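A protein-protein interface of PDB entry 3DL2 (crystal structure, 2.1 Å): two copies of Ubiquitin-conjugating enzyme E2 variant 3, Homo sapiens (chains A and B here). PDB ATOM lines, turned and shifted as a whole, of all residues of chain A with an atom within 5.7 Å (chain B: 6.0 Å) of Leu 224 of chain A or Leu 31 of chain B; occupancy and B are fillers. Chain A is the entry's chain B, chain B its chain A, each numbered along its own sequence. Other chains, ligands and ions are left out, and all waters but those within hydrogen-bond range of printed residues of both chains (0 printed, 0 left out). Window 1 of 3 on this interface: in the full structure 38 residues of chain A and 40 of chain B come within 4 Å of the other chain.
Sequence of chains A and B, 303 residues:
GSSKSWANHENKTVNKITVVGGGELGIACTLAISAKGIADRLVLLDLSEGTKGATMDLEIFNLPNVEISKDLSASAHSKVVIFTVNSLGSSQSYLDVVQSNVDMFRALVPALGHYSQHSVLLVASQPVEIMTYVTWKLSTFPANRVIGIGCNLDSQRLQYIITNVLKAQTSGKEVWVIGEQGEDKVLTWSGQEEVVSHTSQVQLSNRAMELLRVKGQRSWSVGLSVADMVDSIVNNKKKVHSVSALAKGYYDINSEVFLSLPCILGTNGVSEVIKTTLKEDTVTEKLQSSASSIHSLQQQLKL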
ATOM      1  N   ALA A  28       9.047 -19.310 -18.480  1.00  0.00           N
ATOM      2  CA  ALA A  28       9.524 -17.992 -18.909  1.00  0.00           C
ATOM      3  C   ALA A  28       9.569 -16.993 -17.747  1.00  0.00           C
ATOM      4  O   ALA A  28      10.552 -16.265 -17.595  1.00  0.00           O
ATOM      5  CB  ALA A  28       8.669 -17.457 -20.055  1.00  0.00           C
ATOM      6  N   CYS A  29       8.510 -16.974 -16.935  1.00  0.00           N
ATOM      7  CA  CYS A  29       8.457 -16.155 -15.712  1.00  0.00           C
ATOM      8  C   CYS A  29       9.583 -16.543 -14.753  1.00  0.00           C
ATOM      9  O   CYS A  29      10.303 -15.681 -14.264  1.00  0.00           O
ATOM     10  CB  CYS A  29       7.108 -16.307 -15.001  1.00  0.00           C
ATOM     11  SG  CYS A  29       5.698 -15.618 -15.898  1.00  0.00           S
ATOM     12  N   LEU A  31      12.504 -18.153 -15.333  1.00  0.00           N
ATOM     13  CA  LEU A  31      13.821 -17.791 -15.859  1.00  0.00           C
ATOM     14  C   LEU A  31      14.070 -16.285 -15.820  1.00  0.00           C
ATOM     15  O   LEU A  31      15.167 -15.849 -15.458  1.00  0.00           O
ATOM     16  CB  LEU A  31      14.029 -18.330 -17.285  1.00  0.00           C
ATOM     17  CG  LEU A  31      14.273 -19.840 -17.420  1.00  0.00           C
ATOM     18  CD1 LEU A  31      14.454 -20.224 -18.872  1.00  0.00           C
ATOM     19  CD2 LEU A  31      15.479 -20.306 -16.610  1.00  0.00           C
ATOM     20  N   ALA A  32      13.059 -15.499 -16.190  1.00  0.00           N
ATOM     21  CA  ALA A  32      13.180 -14.038 -16.179  1.00  0.00           C
ATOM     22  C   ALA A  32      13.403 -13.500 -14.765  1.00  0.00           C
ATOM     23  O   ALA A  32      14.259 -12.632 -14.550  1.00  0.00           O
ATOM     24  CB  ALA A  32      11.969 -13.391 -16.819  1.00  0.00           C
ATOM     25  N   ALA A  35      16.913 -14.623 -13.679  1.00  0.00           N
ATOM     26  CA  ALA A  35      17.926 -13.873 -14.428  1.00  0.00           C
ATOM     27  C   ALA A  35      18.263 -12.523 -13.797  1.00  0.00           C
ATOM     28  O   ALA A  35      19.410 -12.085 -13.836  1.00  0.00           O
ATOM     29  CB  ALA A  35      17.499 -13.692 -15.872  1.00  0.00           C
ATOM     30  N   SER A 219       5.311 -16.189 -25.095  1.00  0.00           N
ATOM     31  CA  SER A 219       5.536 -16.524 -23.686  1.00  0.00           C
ATOM     32  C   SER A 219       6.763 -15.856 -23.071  1.00  0.00           C
ATOM     33  O   SER A 219       6.681 -15.349 -21.956  1.00  0.00           O
ATOM     34  CB  SER A 219       5.600 -18.041 -23.486  1.00  0.00           C
ATOM     35  OG  SER A 219       4.300 -18.604 -23.553  1.00  0.00           O
ATOM     36  N   TRP A 220       7.882 -15.842 -23.798  1.00  0.00           N
ATOM     37  CA  TRP A 220       9.110 -15.224 -23.291  1.00  0.00           C
ATOM     38  C   TRP A 220       8.945 -13.723 -23.029  1.00  0.00           C
ATOM     39  O   TRP A 220       9.441 -13.212 -22.031  1.00  0.00           O
ATOM     40  CB  TRP A 220      10.318 -15.522 -24.196  1.00  0.00           C
ATOM     41  CG  TRP A 220      10.326 -14.840 -25.543  1.00  0.00           C
ATOM     42  CD1 TRP A 220       9.841 -15.339 -26.720  1.00  0.00           C
ATOM     43  CD2 TRP A 220      10.888 -13.557 -25.855  1.00  0.00           C
ATOM     44  NE1 TRP A 220      10.045 -14.438 -27.738  1.00  0.00           N
ATOM     45  CE2 TRP A 220      10.685 -13.336 -27.235  1.00  0.00           C
ATOM     46  CE3 TRP A 220      11.530 -12.566 -25.099  1.00  0.00           C
ATOM     47  CZ2 TRP A 220      11.107 -12.166 -27.878  1.00  0.00           C
ATOM     48  CZ3 TRP A 220      11.950 -11.403 -25.740  1.00  0.00           C
ATOM     49  CH2 TRP A 220      11.735 -11.216 -27.116  1.00  0.00           C
ATOM     50  N   SER A 221       8.226 -13.036 -23.915  1.00  0.00           N
ATOM     51  CA  SER A 221       7.940 -11.599 -23.753  1.00  0.00           C
ATOM     52  C   SER A 221       7.052 -11.313 -22.542  1.00  0.00           C
ATOM     53  O   SER A 221       7.329 -10.390 -21.763  1.00  0.00           O
ATOM     54  CB  SER A 221       7.284 -11.031 -25.010  1.00  0.00           C
ATOM     55  OG  SER A 221       8.140 -11.153 -26.134  1.00  0.00           O
ATOM     56  N   VAL A 222       5.985 -12.100 -22.394  1.00  0.00           N
ATOM     57  CA  VAL A 222       5.095 -11.985 -21.232  1.00  0.00           C
ATOM     58  C   VAL A 222       5.869 -12.301 -19.937  1.00  0.00           C
ATOM     59  O   VAL A 222       5.697 -11.617 -18.925  1.00  0.00           O
ATOM     60  CB  VAL A 222       3.825 -12.878 -21.375  1.00  0.00           C
ATOM     61  CG1 VAL A 222       2.915 -12.748 -20.142  1.00  0.00           C
ATOM     62  CG2 VAL A 222       3.036 -12.518 -22.661  1.00  0.00           C
ATOM     63  N   GLY A 223       6.726 -13.320 -19.973  1.00  0.00           N
ATOM     64  CA  GLY A 223       7.558 -13.660 -18.812  1.00  0.00           C
ATOM     65  C   GLY A 223       8.417 -12.489 -18.343  1.00  0.00           C
ATOM     66  O   GLY A 223       8.506 -12.210 -17.149  1.00  0.00           O
ATOM     67  N   LEU A 224       9.055 -11.810 -19.292  1.00  0.00           N
ATOM     68  CA  LEU A 224       9.867 -10.626 -18.998  1.00  0.00           C
ATOM     69  C   LEU A 224       9.043  -9.499 -18.378  1.00  0.00           C
ATOM     70  O   LEU A 224       9.470  -8.896 -17.396  1.00  0.00           O
ATOM     71  CB  LEU A 224      10.590 -10.112 -20.253  1.00  0.00           C
ATOM     72  CG  LEU A 224      11.658 -11.003 -20.904  1.00  0.00           C
ATOM     73  CD1 LEU A 224      12.137 -10.403 -22.221  1.00  0.00           C
ATOM     74  CD2 LEU A 224      12.837 -11.235 -19.989  1.00  0.00           C
ATOM     75  N   SER A 225       7.870  -9.214 -18.947  1.00  0.00           N
ATOM     76  CA  SER A 225       7.021  -8.153 -18.405  1.00  0.00           C
ATOM     77  C   SER A 225       6.499  -8.513 -17.016  1.00  0.00           C
ATOM     78  O   SER A 225       6.418  -7.659 -16.146  1.00  0.00           O
ATOM     79  CB  SER A 225       5.863  -7.818 -19.341  1.00  0.00           C
ATOM     80  OG  SER A 225       4.953  -8.891 -19.389  1.00  0.00           O
ATOM     81  N   VAL A 226       6.154  -9.779 -16.808  1.00  0.00           N
ATOM     82  CA  VAL A 226       5.757 -10.250 -15.473  1.00  0.00           C
ATOM     83  C   VAL A 226       6.873 -10.041 -14.443  1.00  0.00           C
ATOM     84  O   VAL A 226       6.637  -9.506 -13.353  1.00  0.00           O
ATOM     85  CB  VAL A 226       5.319 -11.730 -15.501  1.00  0.00           C
ATOM     86  CG1 VAL A 226       5.249 -12.312 -14.076  1.00  0.00           C
ATOM     87  CG2 VAL A 226       3.984 -11.881 -16.227  1.00  0.00           C
ATOM     88  N   ALA A 227       8.088 -10.458 -14.788  1.00  0.00           N
ATOM     89  CA  ALA A 227       9.223 -10.336 -13.874  1.00  0.00           C
ATOM     90  C   ALA A 227       9.446  -8.884 -13.438  1.00  0.00           C
ATOM     91  O   ALA A 227       9.784  -8.625 -12.280  1.00  0.00           O
ATOM     92  CB  ALA A 227      10.486 -10.901 -14.515  1.00  0.00           C
ATOM     93  N   ASP A 228       9.274  -7.953 -14.376  1.00  0.00           N
ATOM     94  CA  ASP A 228       9.422  -6.519 -14.099  1.00  0.00           C
ATOM     95  C   ASP A 228       8.360  -6.016 -13.121  1.00  0.00           C
ATOM     96  O   ASP A 228       8.659  -5.204 -12.239  1.00  0.00           O
ATOM     97  CB  ASP A 228       9.365  -5.692 -15.394  1.00  0.00           C
ATOM     98  CG  ASP A 228       9.729  -4.229 -15.167  1.00  0.00           C
ATOM     99  OD1 ASP A 228      10.828  -3.966 -14.635  1.00  0.00           O
ATOM    100  OD2 ASP A 228       8.919  -3.339 -15.507  1.00  0.00           O
ATOM    101  N   MET A 229       7.124  -6.486 -13.278  1.00  0.00           N
ATOM    102  CA  MET A 229       6.053  -6.124 -12.344  1.00  0.00           C
ATOM    103  C   MET A 229       6.321  -6.681 -10.942  1.00  0.00           C
ATOM    104  O   MET A 229       6.094  -5.997  -9.940  1.00  0.00           O
ATOM    105  CB  MET A 229       4.694  -6.605 -12.853  1.00  0.00           C
ATOM    106  CG  MET A 229       4.112  -5.780 -14.005  1.00  0.00           C
ATOM    107  SD  MET A 229       2.525  -6.450 -14.555  1.00  0.00           S
ATOM    108  CE  MET A 229       3.038  -7.793 -15.596  1.00  0.00           C
ATOM    109  N   GLY B  26      17.337 -18.613 -28.988  1.00  0.00           N
ATOM    110  CA  GLY B  26      18.367 -17.630 -28.614  1.00  0.00           C
ATOM    111  C   GLY B  26      18.014 -16.953 -27.301  1.00  0.00           C
ATOM    112  O   GLY B  26      18.868 -16.764 -26.440  1.00  0.00           O
ATOM    113  N   ILE B  27      16.742 -16.594 -27.155  1.00  0.00           N
ATOM    114  CA  ILE B  27      16.227 -15.985 -25.924  1.00  0.00           C
ATOM    115  C   ILE B  27      16.338 -16.955 -24.734  1.00  0.00           C
ATOM    116  O   ILE B  27      16.762 -16.565 -23.639  1.00  0.00           O
ATOM    117  CB  ILE B  27      14.749 -15.527 -26.103  1.00  0.00           C
ATOM    118  CG1 ILE B  27      14.626 -14.436 -27.185  1.00  0.00           C
ATOM    119  CG2 ILE B  27      14.131 -15.080 -24.767  1.00  0.00           C
ATOM    120  CD1 ILE B  27      15.465 -13.195 -26.950  1.00  0.00           C
ATOM    121  N   ALA B  28      15.957 -18.208 -24.963  1.00  0.00           N
ATOM    122  CA  ALA B  28      16.017 -19.254 -23.937  1.00  0.00           C
ATOM    123  C   ALA B  28      17.442 -19.468 -23.418  1.00  0.00           C
ATOM    124  O   ALA B  28      17.650 -19.574 -22.204  1.00  0.00           O
ATOM    125  CB  ALA B  28      15.439 -20.558 -24.470  1.00  0.00           C
ATOM    126  N   CYS B  29      18.408 -19.532 -24.334  1.00  0.00           N
ATOM    127  CA  CYS B  29      19.831 -19.635 -23.977  1.00  0.00           C
ATOM    128  C   CYS B  29      20.252 -18.429 -23.146  1.00  0.00           C
ATOM    129  O   CYS B  29      20.861 -18.594 -22.098  1.00  0.00           O
ATOM    130  CB  CYS B  29      20.716 -19.727 -25.226  1.00  0.00           C
ATOM    131  SG  CYS B  29      20.556 -21.266 -26.160  1.00  0.00           S
ATOM    132  N   THR B  30      19.897 -17.228 -23.616  1.00  0.00           N
ATOM    133  CA  THR B  30      20.226 -15.969 -22.931  1.00  0.00           C
ATOM    134  C   THR B  30      19.706 -15.924 -21.486  1.00  0.00           C
ATOM    135  O   THR B  30      20.459 -15.589 -20.560  1.00  0.00           O
ATOM    136  CB  THR B  30      19.718 -14.739 -23.729  1.00  0.00           C
ATOM    137  OG1 THR B  30      20.284 -14.756 -25.045  1.00  0.00           O
ATOM    138  CG2 THR B  30      20.109 -13.434 -23.049  1.00  0.00           C
ATOM    139  N   LEU B  31      18.434 -16.276 -21.302  1.00  0.00           N
ATOM    140  CA  LEU B  31      17.806 -16.250 -19.983  1.00  0.00           C
ATOM    141  C   LEU B  31      18.362 -17.319 -19.046  1.00  0.00           C
ATOM    142  O   LEU B  31      18.576 -17.053 -17.860  1.00  0.00           O
ATOM    143  CB  LEU B  31      16.277 -16.362 -20.089  1.00  0.00           C
ATOM    144  CG  LEU B  31      15.537 -15.103 -20.578  1.00  0.00           C
ATOM    145  CD1 LEU B  31      14.052 -15.385 -20.753  1.00  0.00           C
ATOM    146  CD2 LEU B  31      15.726 -13.938 -19.624  1.00  0.00           C
ATOM    147  N   ALA B  32      18.601 -18.518 -19.574  1.00  0.00           N
ATOM    148  CA  ALA B  32      19.172 -19.603 -18.774  1.00  0.00           C
ATOM    149  C   ALA B  32      20.598 -19.281 -18.323  1.00  0.00           C
ATOM    150  O   ALA B  32      20.965 -19.526 -17.167  1.00  0.00           O
ATOM    151  CB  ALA B  32      19.124 -20.924 -19.534  1.00  0.00           C
ATOM    152  N   ILE B  33      21.395 -18.725 -19.231  1.00  0.00           N
ATOM    153  CA  ILE B  33      22.766 -18.313 -18.909  1.00  0.00           C
ATOM    154  C   ILE B  33      22.750 -17.183 -17.873  1.00  0.00           C
ATOM    155  O   ILE B  33      23.512 -17.215 -16.906  1.00  0.00           O
ATOM    156  CB  ILE B  33      23.564 -17.919 -20.184  1.00  0.00           C
ATOM    157  CG1 ILE B  33      23.876 -19.173 -21.011  1.00  0.00           C
ATOM    158  CG2 ILE B  33      24.875 -17.185 -19.824  1.00  0.00           C
ATOM    159  CD1 ILE B  33      24.316 -18.886 -22.437  1.00  0.00           C
ATOM    160  N   SER B  34      21.863 -16.207 -18.068  1.00  0.00           N
ATOM    161  CA  SER B  34      21.717 -15.089 -17.133  1.00  0.00           C
ATOM    162  C   SER B  34      21.206 -15.545 -15.767  1.00  0.00           C
ATOM    163  O   SER B  34      21.704 -15.088 -14.738  1.00  0.00           O
ATOM    164  CB  SER B  34      20.792 -14.013 -17.707  1.00  0.00           C
ATOM    165  OG  SER B  34      21.267 -13.586 -18.971  1.00  0.00           O
ATOM    166  N   ALA B  35      20.230 -16.452 -15.768  1.00  0.00           N
ATOM    167  CA  ALA B  35      19.650 -16.996 -14.532  1.00  0.00           C
ATOM    168  C   ALA B  35      20.691 -17.592 -13.589  1.00  0.00           C
ATOM    169  O   ALA B  35      20.557 -17.499 -12.370  1.00  0.00           O
ATOM    170  CB  ALA B  35      18.578 -18.025 -14.854  1.00  0.00           C
ATOM    171  N   LYS B  36      21.729 -18.202 -14.154  1.00  0.00           N
ATOM    172  CA  LYS B  36      22.757 -18.840 -13.347  1.00  0.00           C
ATOM    173  C   LYS B  36      24.010 -17.982 -13.144  1.00  0.00           C
ATOM    174  O   LYS B  36      24.921 -18.372 -12.408  1.00  0.00           O
ATOM    175  CB  LYS B  36      23.120 -20.208 -13.932  1.00  0.00           C
ATOM    176  CG  LYS B  36      22.427 -21.363 -13.245  1.00  0.00           C
ATOM    177  CD  LYS B  36      23.087 -22.692 -13.584  1.00  0.00           C
ATOM    178  CE  LYS B  36      22.692 -23.753 -12.584  1.00  0.00           C
ATOM    179  NZ  LYS B  36      23.185 -25.101 -12.992  1.00  0.00           N
ATOM    180  N   ASP B  57      11.794  -6.602 -26.404  1.00  0.00           N
ATOM    181  CA  ASP B  57      11.400  -6.885 -25.022  1.00  0.00           C
ATOM    182  C   ASP B  57      12.604  -7.132 -24.112  1.00  0.00           C
ATOM    183  O   ASP B  57      12.598  -6.742 -22.943  1.00  0.00           O
ATOM    184  CB  ASP B  57      10.429  -8.069 -24.975  1.00  0.00           C
ATOM    185  CG  ASP B  57       9.166  -7.815 -25.778  1.00  0.00           C
ATOM    186  OD1 ASP B  57       8.589  -6.711 -25.662  1.00  0.00           O
ATOM    187  OD2 ASP B  57       8.748  -8.724 -26.529  1.00  0.00           O
ATOM    188  N   LEU B  58      13.633  -7.775 -24.660  1.00  0.00           N
ATOM    189  CA  LEU B  58      14.870  -8.018 -23.926  1.00  0.00           C
ATOM    190  C   LEU B  58      15.645  -6.719 -23.667  1.00  0.00           C
ATOM    191  O   LEU B  58      16.232  -6.548 -22.596  1.00  0.00           O
ATOM    192  CB  LEU B  58      15.731  -9.051 -24.660  1.00  0.00           C
ATOM    193  CG  LEU B  58      16.787  -9.813 -23.865  1.00  0.00           C
ATOM    194  CD1 LEU B  58      16.199 -10.567 -22.665  1.00  0.00           C
ATOM    195  CD2 LEU B  58      17.501 -10.770 -24.785  1.00  0.00           C
ATOM    196  N   PHE B  61      13.616  -5.004 -20.870  1.00  0.00           N
ATOM    197  CA  PHE B  61      13.917  -5.713 -19.615  1.00  0.00           C
ATOM    198  C   PHE B  61      15.286  -5.361 -19.043  1.00  0.00           C
ATOM    199  O   PHE B  61      15.473  -5.393 -17.831  1.00  0.00           O
ATOM    200  CB  PHE B  61      13.831  -7.234 -19.820  1.00  0.00           C
ATOM    201  CG  PHE B  61      13.759  -8.034 -18.534  1.00  0.00           C
ATOM    202  CD1 PHE B  61      12.763  -7.785 -17.585  1.00  0.00           C
ATOM    203  CD2 PHE B  61      14.667  -9.065 -18.288  1.00  0.00           C
ATOM    204  CE1 PHE B  61      12.685  -8.536 -16.400  1.00  0.00           C
ATOM    205  CE2 PHE B  61      14.597  -9.827 -17.103  1.00  0.00           C
ATOM    206  CZ  PHE B  61      13.602  -9.561 -16.164  1.00  0.00           C
ATOM    207  N   LEU B  63      18.713  -6.549 -18.906  1.00  0.00           N
ATOM    208  CA  LEU B  63      19.568  -7.381 -18.052  1.00  0.00           C
ATOM    209  C   LEU B  63      20.963  -6.763 -17.912  1.00  0.00           C
ATOM    210  O   LEU B  63      21.564  -6.360 -18.915  1.00  0.00           O
ATOM    211  CB  LEU B  63      19.650  -8.810 -18.587  1.00  0.00           C
ATOM    212  CG  LEU B  63      18.364  -9.634 -18.468  1.00  0.00           C
ATOM    213  CD1 LEU B  63      18.336 -10.751 -19.500  1.00  0.00           C
ATOM    214  CD2 LEU B  63      18.204 -10.179 -17.058  1.00  0.00           C
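OD2 of Asp 57 of chain B is in hydrogen-bond range of OG of Ser 221 of chain A.
Ala 35 of chain A touches its own counterpart, Ala 35 of chain B. Positions printed for both chains: 28, 29, 31, 32 and 35. Of the 12 pairs that touch across the chains among the printed residues, 1 has its exchanged pair printed and touching as well.
Leu 224 of chain A touches just these residues of chain B: Leu 31 (3.97 Å), Asp 57 (3.8 Å), Leu 58 (3.9 Å) and Phe 61 (3.3 Å). Printed residues of chain A within 4 Å of Leu 31 of chain B: Leu 224 (3.97 Å). Of the printed residues of chain B, Ala 35 of chain A touches Ser 34 (3.8 Å), Ala 35 (3.6 Å) and Leu 63 (3.8 Å). Printed residues of chain A within 4 Å of Ala 35 of chain B: Ala 35. Printed residues of chain B within 4 Å of Ala 32 of chain A: Phe 61. Of the printed residues of chain A, Asp 57 of chain B touches Trp 220 (3.7 Å), Ser 221 (2.5 Å) and Leu 224 (3.8 Å). Of the printed residues of chain A, Phe 61 of chain B touches Ala 32 (3.5 Å), Leu 224 (3.3 Å) and Ala 227 (3.7 Å). Ile 33 of chain B touches none of the printed residues of chain A. Thr 30 of chain B touches none of the printed residues of chain A. The nearest printed residue of chain A that does not touch Leu 31 of chain B is Ala 35 of chain A (4.1 Å).
O of Thr 30 of chain B is in hydrogen-bond range of OG of Ser 34 of chain B (2.7 Å).
Printed residues of chain A that touch a printed residue of chain B: Ala 32, Ala 35, Trp 220, Ser 221, Leu 224 and Ala 227. Hydrophobic or aromatic side chains of chain A within 4 Å of the printed part of chain B: Ala 35, Trp 220, Leu 224 and Ala 227. Of the 15 printed residues of chain B, 8 touch a printed residue of chain A. Along chain B the printed residues that touch a printed residue of chain A span positions 27 to 63. Among the printed residues, no Asp or Glu carboxylate lies within 4 Å of a Lys or Arg side-chain nitrogen of the other chain.
O of Ala 32 of chain A touches CZ of Phe 61 of chain B, 3.5 Å away. Ser 34 of chain B touches Ala 35 of chain A (CB to CB, 3.8 Å). Leu 63 of chain B touches Ala 35 of chain A. CG2 of Ile 27 of chain B touches CE3 of Trp 220 of chain A (3.6 Å). CZ3 of Trp 220 of chain A touches CB of Asp 57 of chain B (3.7 Å). Leu 31 of chain B touches Leu 224 of chain A (CD2 to CD2, 3.97 Å). Leu 224 of chain A touches Asp 57 of chain B (CD1 to O, 3.8 Å). N of Leu 58 of chain B touches CD1 of Leu 224 of chain A, at 3.9 Å. Phe 61 of chain B touches Leu 224 of chain A. Phe 61 of chain B touches Ala 227 of chain A.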
